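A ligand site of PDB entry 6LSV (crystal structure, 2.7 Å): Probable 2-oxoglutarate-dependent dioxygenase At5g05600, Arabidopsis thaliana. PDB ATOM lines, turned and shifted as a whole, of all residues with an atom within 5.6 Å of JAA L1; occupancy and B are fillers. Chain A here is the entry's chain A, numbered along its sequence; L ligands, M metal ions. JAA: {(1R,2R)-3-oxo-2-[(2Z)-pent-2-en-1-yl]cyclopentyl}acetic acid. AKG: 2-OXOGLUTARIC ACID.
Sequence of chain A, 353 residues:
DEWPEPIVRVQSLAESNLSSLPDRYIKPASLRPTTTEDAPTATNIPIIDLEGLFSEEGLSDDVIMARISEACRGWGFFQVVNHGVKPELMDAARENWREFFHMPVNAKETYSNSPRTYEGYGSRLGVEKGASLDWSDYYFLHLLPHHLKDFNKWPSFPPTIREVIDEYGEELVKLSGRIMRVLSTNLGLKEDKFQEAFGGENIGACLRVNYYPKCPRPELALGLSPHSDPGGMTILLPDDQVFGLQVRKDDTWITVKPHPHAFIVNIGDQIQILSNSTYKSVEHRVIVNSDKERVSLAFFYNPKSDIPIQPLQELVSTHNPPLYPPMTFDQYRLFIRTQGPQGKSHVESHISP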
ATOM      1  N   THR A 117      12.658  -5.781  11.240  1.00  0.00           N
ATOM      2  CA  THR A 117      13.821  -5.762  10.368  1.00  0.00           C
ATOM      3  C   THR A 117      13.478  -5.620   8.898  1.00  0.00           C
ATOM      4  O   THR A 117      14.364  -5.260   8.103  1.00  0.00           O
ATOM      5  CB  THR A 117      14.684  -7.018  10.538  1.00  0.00           C
ATOM      6  OG1 THR A 117      14.001  -8.150  10.002  1.00  0.00           O
ATOM      7  CG2 THR A 117      15.001  -7.273  12.008  1.00  0.00           C
ATOM      8  N   TYR A 118      12.237  -5.908   8.498  1.00  0.00           N
ATOM      9  CA  TYR A 118      11.762  -5.795   7.126  1.00  0.00           C
ATOM     10  C   TYR A 118      12.474  -6.778   6.188  1.00  0.00           C
ATOM     11  O   TYR A 118      12.153  -6.839   4.998  1.00  0.00           O
ATOM     12  CB  TYR A 118      11.909  -4.361   6.613  1.00  0.00           C
ATOM     13  CG  TYR A 118      10.710  -3.486   6.883  1.00  0.00           C
ATOM     14  CD1 TYR A 118       9.622  -3.467   6.019  1.00  0.00           C
ATOM     15  CD2 TYR A 118      10.670  -2.665   8.005  1.00  0.00           C
ATOM     16  CE1 TYR A 118       8.524  -2.665   6.267  1.00  0.00           C
ATOM     17  CE2 TYR A 118       9.574  -1.854   8.264  1.00  0.00           C
ATOM     18  CZ  TYR A 118       8.504  -1.857   7.387  1.00  0.00           C
ATOM     19  OH  TYR A 118       7.414  -1.050   7.630  1.00  0.00           O
ATOM     20  N   LEU A 125       4.937  -1.251   3.187  1.00  0.00           N
ATOM     21  CA  LEU A 125       5.936  -0.488   3.931  1.00  0.00           C
ATOM     22  C   LEU A 125       5.190   0.479   4.832  1.00  0.00           C
ATOM     23  O   LEU A 125       4.425   1.324   4.349  1.00  0.00           O
ATOM     24  CB  LEU A 125       6.874   0.245   2.967  1.00  0.00           C
ATOM     25  CG  LEU A 125       8.009   1.128   3.492  1.00  0.00           C
ATOM     26  CD1 LEU A 125       8.886   0.375   4.474  1.00  0.00           C
ATOM     27  CD2 LEU A 125       8.838   1.634   2.322  1.00  0.00           C
ATOM     28  N   TYR A 138       7.846  -7.083  -2.857  1.00  0.00           N
ATOM     29  CA  TYR A 138       9.267  -6.757  -2.838  1.00  0.00           C
ATOM     30  C   TYR A 138      10.007  -7.746  -1.956  1.00  0.00           C
ATOM     31  O   TYR A 138       9.408  -8.476  -1.156  1.00  0.00           O
ATOM     32  CB  TYR A 138       9.506  -5.319  -2.363  1.00  0.00           C
ATOM     33  CG  TYR A 138       9.174  -5.099  -0.910  1.00  0.00           C
ATOM     34  CD1 TYR A 138      10.136  -5.276   0.080  1.00  0.00           C
ATOM     35  CD2 TYR A 138       7.898  -4.708  -0.522  1.00  0.00           C
ATOM     36  CE1 TYR A 138       9.841  -5.085   1.408  1.00  0.00           C
ATOM     37  CE2 TYR A 138       7.587  -4.503   0.817  1.00  0.00           C
ATOM     38  CZ  TYR A 138       8.559  -4.690   1.775  1.00  0.00           C
ATOM     39  OH  TYR A 138       8.270  -4.498   3.111  1.00  0.00           O
ATOM     40  N   PHE A 140      13.674  -7.711   0.572  1.00  0.00           N
ATOM     41  CA  PHE A 140      14.648  -6.831   1.217  1.00  0.00           C
ATOM     42  C   PHE A 140      15.673  -7.670   1.969  1.00  0.00           C
ATOM     43  O   PHE A 140      15.309  -8.619   2.668  1.00  0.00           O
ATOM     44  CB  PHE A 140      13.941  -5.848   2.164  1.00  0.00           C
ATOM     45  CG  PHE A 140      14.860  -4.892   2.857  1.00  0.00           C
ATOM     46  CD1 PHE A 140      15.538  -3.915   2.148  1.00  0.00           C
ATOM     47  CD2 PHE A 140      15.046  -4.974   4.229  1.00  0.00           C
ATOM     48  CE1 PHE A 140      16.376  -3.030   2.805  1.00  0.00           C
ATOM     49  CE2 PHE A 140      15.884  -4.089   4.886  1.00  0.00           C
ATOM     50  CZ  PHE A 140      16.556  -3.113   4.169  1.00  0.00           C
ATOM     51  N   CYS A 206      22.323  -2.337   1.507  1.00  0.00           N
ATOM     52  CA  CYS A 206      21.195  -3.245   1.450  1.00  0.00           C
ATOM     53  C   CYS A 206      20.595  -3.235   0.051  1.00  0.00           C
ATOM     54  O   CYS A 206      20.933  -2.402  -0.798  1.00  0.00           O
ATOM     55  CB  CYS A 206      20.141  -2.910   2.523  1.00  0.00           C
ATOM     56  SG  CYS A 206      19.838  -1.159   2.798  1.00  0.00           S
ATOM     57  N   ARG A 208      16.864  -3.940  -2.149  1.00  0.00           N
ATOM     58  CA  ARG A 208      15.429  -4.151  -2.237  1.00  0.00           C
ATOM     59  C   ARG A 208      15.066  -4.349  -3.688  1.00  0.00           C
ATOM     60  O   ARG A 208      15.352  -3.487  -4.525  1.00  0.00           O
ATOM     61  CB  ARG A 208      14.631  -2.987  -1.642  1.00  0.00           C
ATOM     62  CG  ARG A 208      13.213  -2.917  -2.191  1.00  0.00           C
ATOM     63  CD  ARG A 208      12.251  -2.194  -1.280  1.00  0.00           C
ATOM     64  NE  ARG A 208      10.976  -1.971  -1.955  1.00  0.00           N
ATOM     65  CZ  ARG A 208       9.821  -1.735  -1.338  1.00  0.00           C
ATOM     66  NH1 ARG A 208       9.780  -1.701  -0.015  1.00  0.00           N
ATOM     67  NH2 ARG A 208       8.714  -1.533  -2.035  1.00  0.00           N
ATOM     68  N   LEU A 224       4.475   2.066  -6.642  1.00  0.00           N
ATOM     69  CA  LEU A 224       5.159   2.569  -5.456  1.00  0.00           C
ATOM     70  C   LEU A 224       4.858   4.061  -5.342  1.00  0.00           C
ATOM     71  O   LEU A 224       5.122   4.826  -6.270  1.00  0.00           O
ATOM     72  CB  LEU A 224       6.662   2.321  -5.557  1.00  0.00           C
ATOM     73  CG  LEU A 224       7.486   2.432  -4.280  1.00  0.00           C
ATOM     74  CD1 LEU A 224       6.834   1.663  -3.140  1.00  0.00           C
ATOM     75  CD2 LEU A 224       8.902   1.932  -4.542  1.00  0.00           C
ATOM     76  N   HIS A 227       8.170   9.107  -2.930  1.00  0.00           N
ATOM     77  CA  HIS A 227       9.122   9.097  -1.829  1.00  0.00           C
ATOM     78  C   HIS A 227      10.499   9.467  -2.365  1.00  0.00           C
ATOM     79  O   HIS A 227      10.785   9.314  -3.563  1.00  0.00           O
ATOM     80  CB  HIS A 227       9.203   7.738  -1.139  1.00  0.00           C
ATOM     81  CG  HIS A 227       9.912   6.695  -1.948  1.00  0.00           C
ATOM     82  ND1 HIS A 227       9.412   6.221  -3.148  1.00  0.00           N
ATOM     83  CD2 HIS A 227      11.079   6.059  -1.745  1.00  0.00           C
ATOM     84  CE1 HIS A 227      10.248   5.328  -3.647  1.00  0.00           C
ATOM     85  NE2 HIS A 227      11.266   5.207  -2.813  1.00  0.00           N
ATOM     86  N   ASP A 229      14.526   8.298  -1.275  1.00  0.00           N
ATOM     87  CA  ASP A 229      15.169   7.218  -0.540  1.00  0.00           C
ATOM     88  C   ASP A 229      15.790   7.756   0.742  1.00  0.00           C
ATOM     89  O   ASP A 229      16.484   8.781   0.702  1.00  0.00           O
ATOM     90  CB  ASP A 229      16.226   6.548  -1.412  1.00  0.00           C
ATOM     91  CG  ASP A 229      15.615   5.828  -2.594  1.00  0.00           C
ATOM     92  OD1 ASP A 229      14.505   5.289  -2.445  1.00  0.00           O
ATOM     93  OD2 ASP A 229      16.250   5.806  -3.670  1.00  0.00           O
ATOM     94  N   PRO A 230      15.569   7.109   1.881  1.00  0.00           N
ATOM     95  CA  PRO A 230      16.066   7.674   3.154  1.00  0.00           C
ATOM     96  C   PRO A 230      17.582   7.652   3.279  1.00  0.00           C
ATOM     97  O   PRO A 230      18.132   8.497   3.990  1.00  0.00           O
ATOM     98  CB  PRO A 230      15.402   6.777   4.208  1.00  0.00           C
ATOM     99  CG  PRO A 230      15.092   5.506   3.504  1.00  0.00           C
ATOM    100  CD  PRO A 230      14.794   5.870   2.077  1.00  0.00           C
ATOM    101  N   PHE A 300      20.982   0.158  -2.039  1.00  0.00           N
ATOM    102  CA  PHE A 300      21.088   1.297  -1.140  1.00  0.00           C
ATOM    103  C   PHE A 300      22.490   1.340  -0.535  1.00  0.00           C
ATOM    104  O   PHE A 300      22.929   0.371   0.084  1.00  0.00           O
ATOM    105  CB  PHE A 300      20.035   1.229  -0.037  1.00  0.00           C
ATOM    106  CG  PHE A 300      18.626   1.108  -0.533  1.00  0.00           C
ATOM    107  CD1 PHE A 300      18.056   2.118  -1.305  1.00  0.00           C
ATOM    108  CD2 PHE A 300      17.867  -0.007  -0.230  1.00  0.00           C
ATOM    109  CE1 PHE A 300      16.742   2.005  -1.761  1.00  0.00           C
ATOM    110  CE2 PHE A 300      16.566  -0.115  -0.683  1.00  0.00           C
ATOM    111  CZ  PHE A 300      16.006   0.886  -1.450  1.00  0.00           C
ATOM    112  N   ASN A 302      24.520   3.267   2.203  1.00  0.00           N
ATOM    113  CA  ASN A 302      24.104   4.081   3.329  1.00  0.00           C
ATOM    114  C   ASN A 302      25.258   4.374   4.266  1.00  0.00           C
ATOM    115  O   ASN A 302      26.227   3.620   4.334  1.00  0.00           O
ATOM    116  CB  ASN A 302      22.987   3.363   4.113  1.00  0.00           C
ATOM    117  CG  ASN A 302      21.759   3.114   3.265  1.00  0.00           C
ATOM    118  OD1 ASN A 302      21.398   3.924   2.410  1.00  0.00           O
ATOM    119  ND2 ASN A 302      21.112   1.970   3.486  1.00  0.00           N
ATOM    120  N   PHE A 329      21.241   7.528  11.070  1.00  0.00           N
ATOM    121  CA  PHE A 329      20.405   6.868  10.089  1.00  0.00           C
ATOM    122  C   PHE A 329      19.527   5.792  10.714  1.00  0.00           C
ATOM    123  O   PHE A 329      18.479   5.462  10.160  1.00  0.00           O
ATOM    124  CB  PHE A 329      21.265   6.257   8.974  1.00  0.00           C
ATOM    125  CG  PHE A 329      20.471   5.667   7.848  1.00  0.00           C
ATOM    126  CD1 PHE A 329      19.495   6.416   7.213  1.00  0.00           C
ATOM    127  CD2 PHE A 329      20.689   4.367   7.438  1.00  0.00           C
ATOM    128  CE1 PHE A 329      18.757   5.871   6.179  1.00  0.00           C
ATOM    129  CE2 PHE A 329      19.961   3.813   6.410  1.00  0.00           C
ATOM    130  CZ  PHE A 329      18.982   4.571   5.778  1.00  0.00           C
ATOM    131  N   ARG A 333      15.680   6.195   9.503  1.00  0.00           N
ATOM    132  CA  ARG A 333      14.999   5.186   8.686  1.00  0.00           C
ATOM    133  C   ARG A 333      13.692   4.713   9.300  1.00  0.00           C
ATOM    134  O   ARG A 333      12.897   4.088   8.586  1.00  0.00           O
ATOM    135  CB  ARG A 333      15.937   4.008   8.449  1.00  0.00           C
ATOM    136  CG  ARG A 333      16.103   3.115   9.663  1.00  0.00           C
ATOM    137  CD  ARG A 333      17.405   2.361   9.609  1.00  0.00           C
ATOM    138  NE  ARG A 333      17.619   1.769   8.298  1.00  0.00           N
ATOM    139  CZ  ARG A 333      18.693   1.068   7.975  1.00  0.00           C
ATOM    140  NH1 ARG A 333      19.654   0.879   8.880  1.00  0.00           N
ATOM    141  NH2 ARG A 333      18.829   0.551   6.755  1.00  0.00           N
ATOM    142  N   ILE A 336      10.156   6.148   7.412  1.00  0.00           N
ATOM    143  CA  ILE A 336       9.534   5.408   6.328  1.00  0.00           C
ATOM    144  C   ILE A 336       9.167   3.997   6.778  1.00  0.00           C
ATOM    145  O   ILE A 336       8.263   3.372   6.219  1.00  0.00           O
ATOM    146  CB  ILE A 336      10.442   5.383   5.087  1.00  0.00           C
ATOM    147  CG1 ILE A 336       9.600   5.298   3.809  1.00  0.00           C
ATOM    148  CG2 ILE A 336      11.442   4.227   5.151  1.00  0.00           C
ATOM    149  CD1 ILE A 336      10.411   5.264   2.529  1.00  0.00           C
ATOM    150  N   ARG A 337       9.857   3.466   7.799  1.00  0.00           N
ATOM    151  CA  ARG A 337       9.496   2.137   8.291  1.00  0.00           C
ATOM    152  C   ARG A 337       8.154   2.158   9.019  1.00  0.00           C
ATOM    153  O   ARG A 337       7.428   1.171   8.993  1.00  0.00           O
ATOM    154  CB  ARG A 337      10.589   1.599   9.202  1.00  0.00           C
ATOM    155  CG  ARG A 337      11.705   0.908   8.462  1.00  0.00           C
ATOM    156  CD  ARG A 337      12.966   0.813   9.302  1.00  0.00           C
ATOM    157  NE  ARG A 337      14.059   0.175   8.576  1.00  0.00           N
ATOM    158  CZ  ARG A 337      14.617  -0.985   8.930  1.00  0.00           C
ATOM    159  NH1 ARG A 337      14.190  -1.627  10.009  1.00  0.00           N
ATOM    160  NH2 ARG A 337      15.604  -1.488   8.201  1.00  0.00           N
ATOM    161  N   PRO A 341       5.925   5.278   2.281  1.00  0.00           N
ATOM    162  CA  PRO A 341       6.200   6.426   1.413  1.00  0.00           C
ATOM    163  C   PRO A 341       5.375   7.663   1.738  1.00  0.00           C
ATOM    164  O   PRO A 341       4.142   7.614   1.755  1.00  0.00           O
ATOM    165  CB  PRO A 341       5.854   5.894   0.015  1.00  0.00           C
ATOM    166  CG  PRO A 341       6.077   4.431   0.120  1.00  0.00           C
ATOM    167  CD  PRO A 341       5.649   4.051   1.511  1.00  0.00           C
HETATM  168  O01 JAA L   1      11.972  -1.585   1.993  1.00  0.00           O
HETATM  169  O02 JAA L   1      16.850   1.138   5.029  1.00  0.00           O
HETATM  170  O03 JAA L   1      15.414   1.231   6.655  1.00  0.00           O
HETATM  171  C04 JAA L   1      14.210   0.176   3.827  1.00  0.00           C
HETATM  172  C05 JAA L   1      12.916   0.252   2.837  1.00  0.00           C
HETATM  173  C06 JAA L   1      13.764  -0.830   4.925  1.00  0.00           C
HETATM  174  C07 JAA L   1      12.666  -1.500   4.424  1.00  0.00           C
HETATM  175  C08 JAA L   1      12.456  -0.966   2.887  1.00  0.00           C
HETATM  176  C09 JAA L   1      13.337   0.643   1.352  1.00  0.00           C
HETATM  177  C10 JAA L   1      14.526   1.440   4.403  1.00  0.00           C
HETATM  178  C11 JAA L   1      13.364   2.162   1.196  1.00  0.00           C
HETATM  179  C12 JAA L   1      15.660   1.264   5.415  1.00  0.00           C
HETATM  180  C13 JAA L   1      12.763   2.772   0.192  1.00  0.00           C
HETATM  181  C14 JAA L   1      12.011   1.983  -0.881  1.00  0.00           C
HETATM  182  C15 JAA L   1      10.602   2.546  -1.038  1.00  0.00           C
HETATM  183  C1  AKG L   2      12.833   1.977  -5.392  1.00  0.00           C
HETATM  184  O1  AKG L   2      13.833   2.649  -5.055  1.00  0.00           O
HETATM  185  O2  AKG L   2      12.431   1.041  -4.640  1.00  0.00           O
HETATM  186  C2  AKG L   2      12.099   2.306  -6.695  1.00  0.00           C
HETATM  187  O5  AKG L   2      11.596   3.379  -6.810  1.00  0.00           O
HETATM  188  C3  AKG L   2      11.986   1.304  -7.856  1.00  0.00           C
HETATM  189  C4  AKG L   2      12.087   2.064  -9.186  1.00  0.00           C
HETATM  190  C5  AKG L   2      11.552   1.213 -10.343  1.00  0.00           C
HETATM  191  O3  AKG L   2      11.995   1.358 -11.509  1.00  0.00           O
HETATM  192  O4  AKG L   2      10.664   0.356 -10.119  1.00  0.00           O
HETATM  193 FE    FE M   1      13.044   4.252  -4.115  1.00  0.00          FE
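The backbone NH (N) of Phe 300 lies within hydrogen-bond range of the backbone carbonyl oxygen (O) of Cys 206 (2.8 Å).
O of Arg 337 sits at hydrogen-bond distance from OH of Tyr 118 (2.6 Å).
Tyr 118 touches JAA L1 (CB to C07, 3.7 Å).
CD2 of Leu 125 touches C15 of JAA L1, at 3.9 Å.
CZ of Phe 140 touches C06 of JAA L1 (3.7 Å).
Leu 224 touches JAA L1.
His 227 touches JAA L1 (NE2 to C15, 3.3 Å).
Phe 300 touches JAA L1.
Within 4 Å of JAA L1: Tyr 118, Leu 125, Phe 140, Arg 208, Leu 224, His 227, Phe 300, Arg 333 and Arg 337.
The nearest printed residue that does not touch JAA L1 is Asp 229 (4.04 Å).
The guanidinium group (NH2) of Arg 333 lies within salt-bridge range of an oxygen (O02) of JAA L1 (2.7 Å).
An oxygen (O03) of JAA L1 is in salt-bridge range of the guanidinium group of Arg 337, at 2.6 Å.
An oxygen (O01) of JAA L1 sits at hydrogen-bond distance from the guanidinium group (NH1) of Arg 208, at 3.0 Å.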
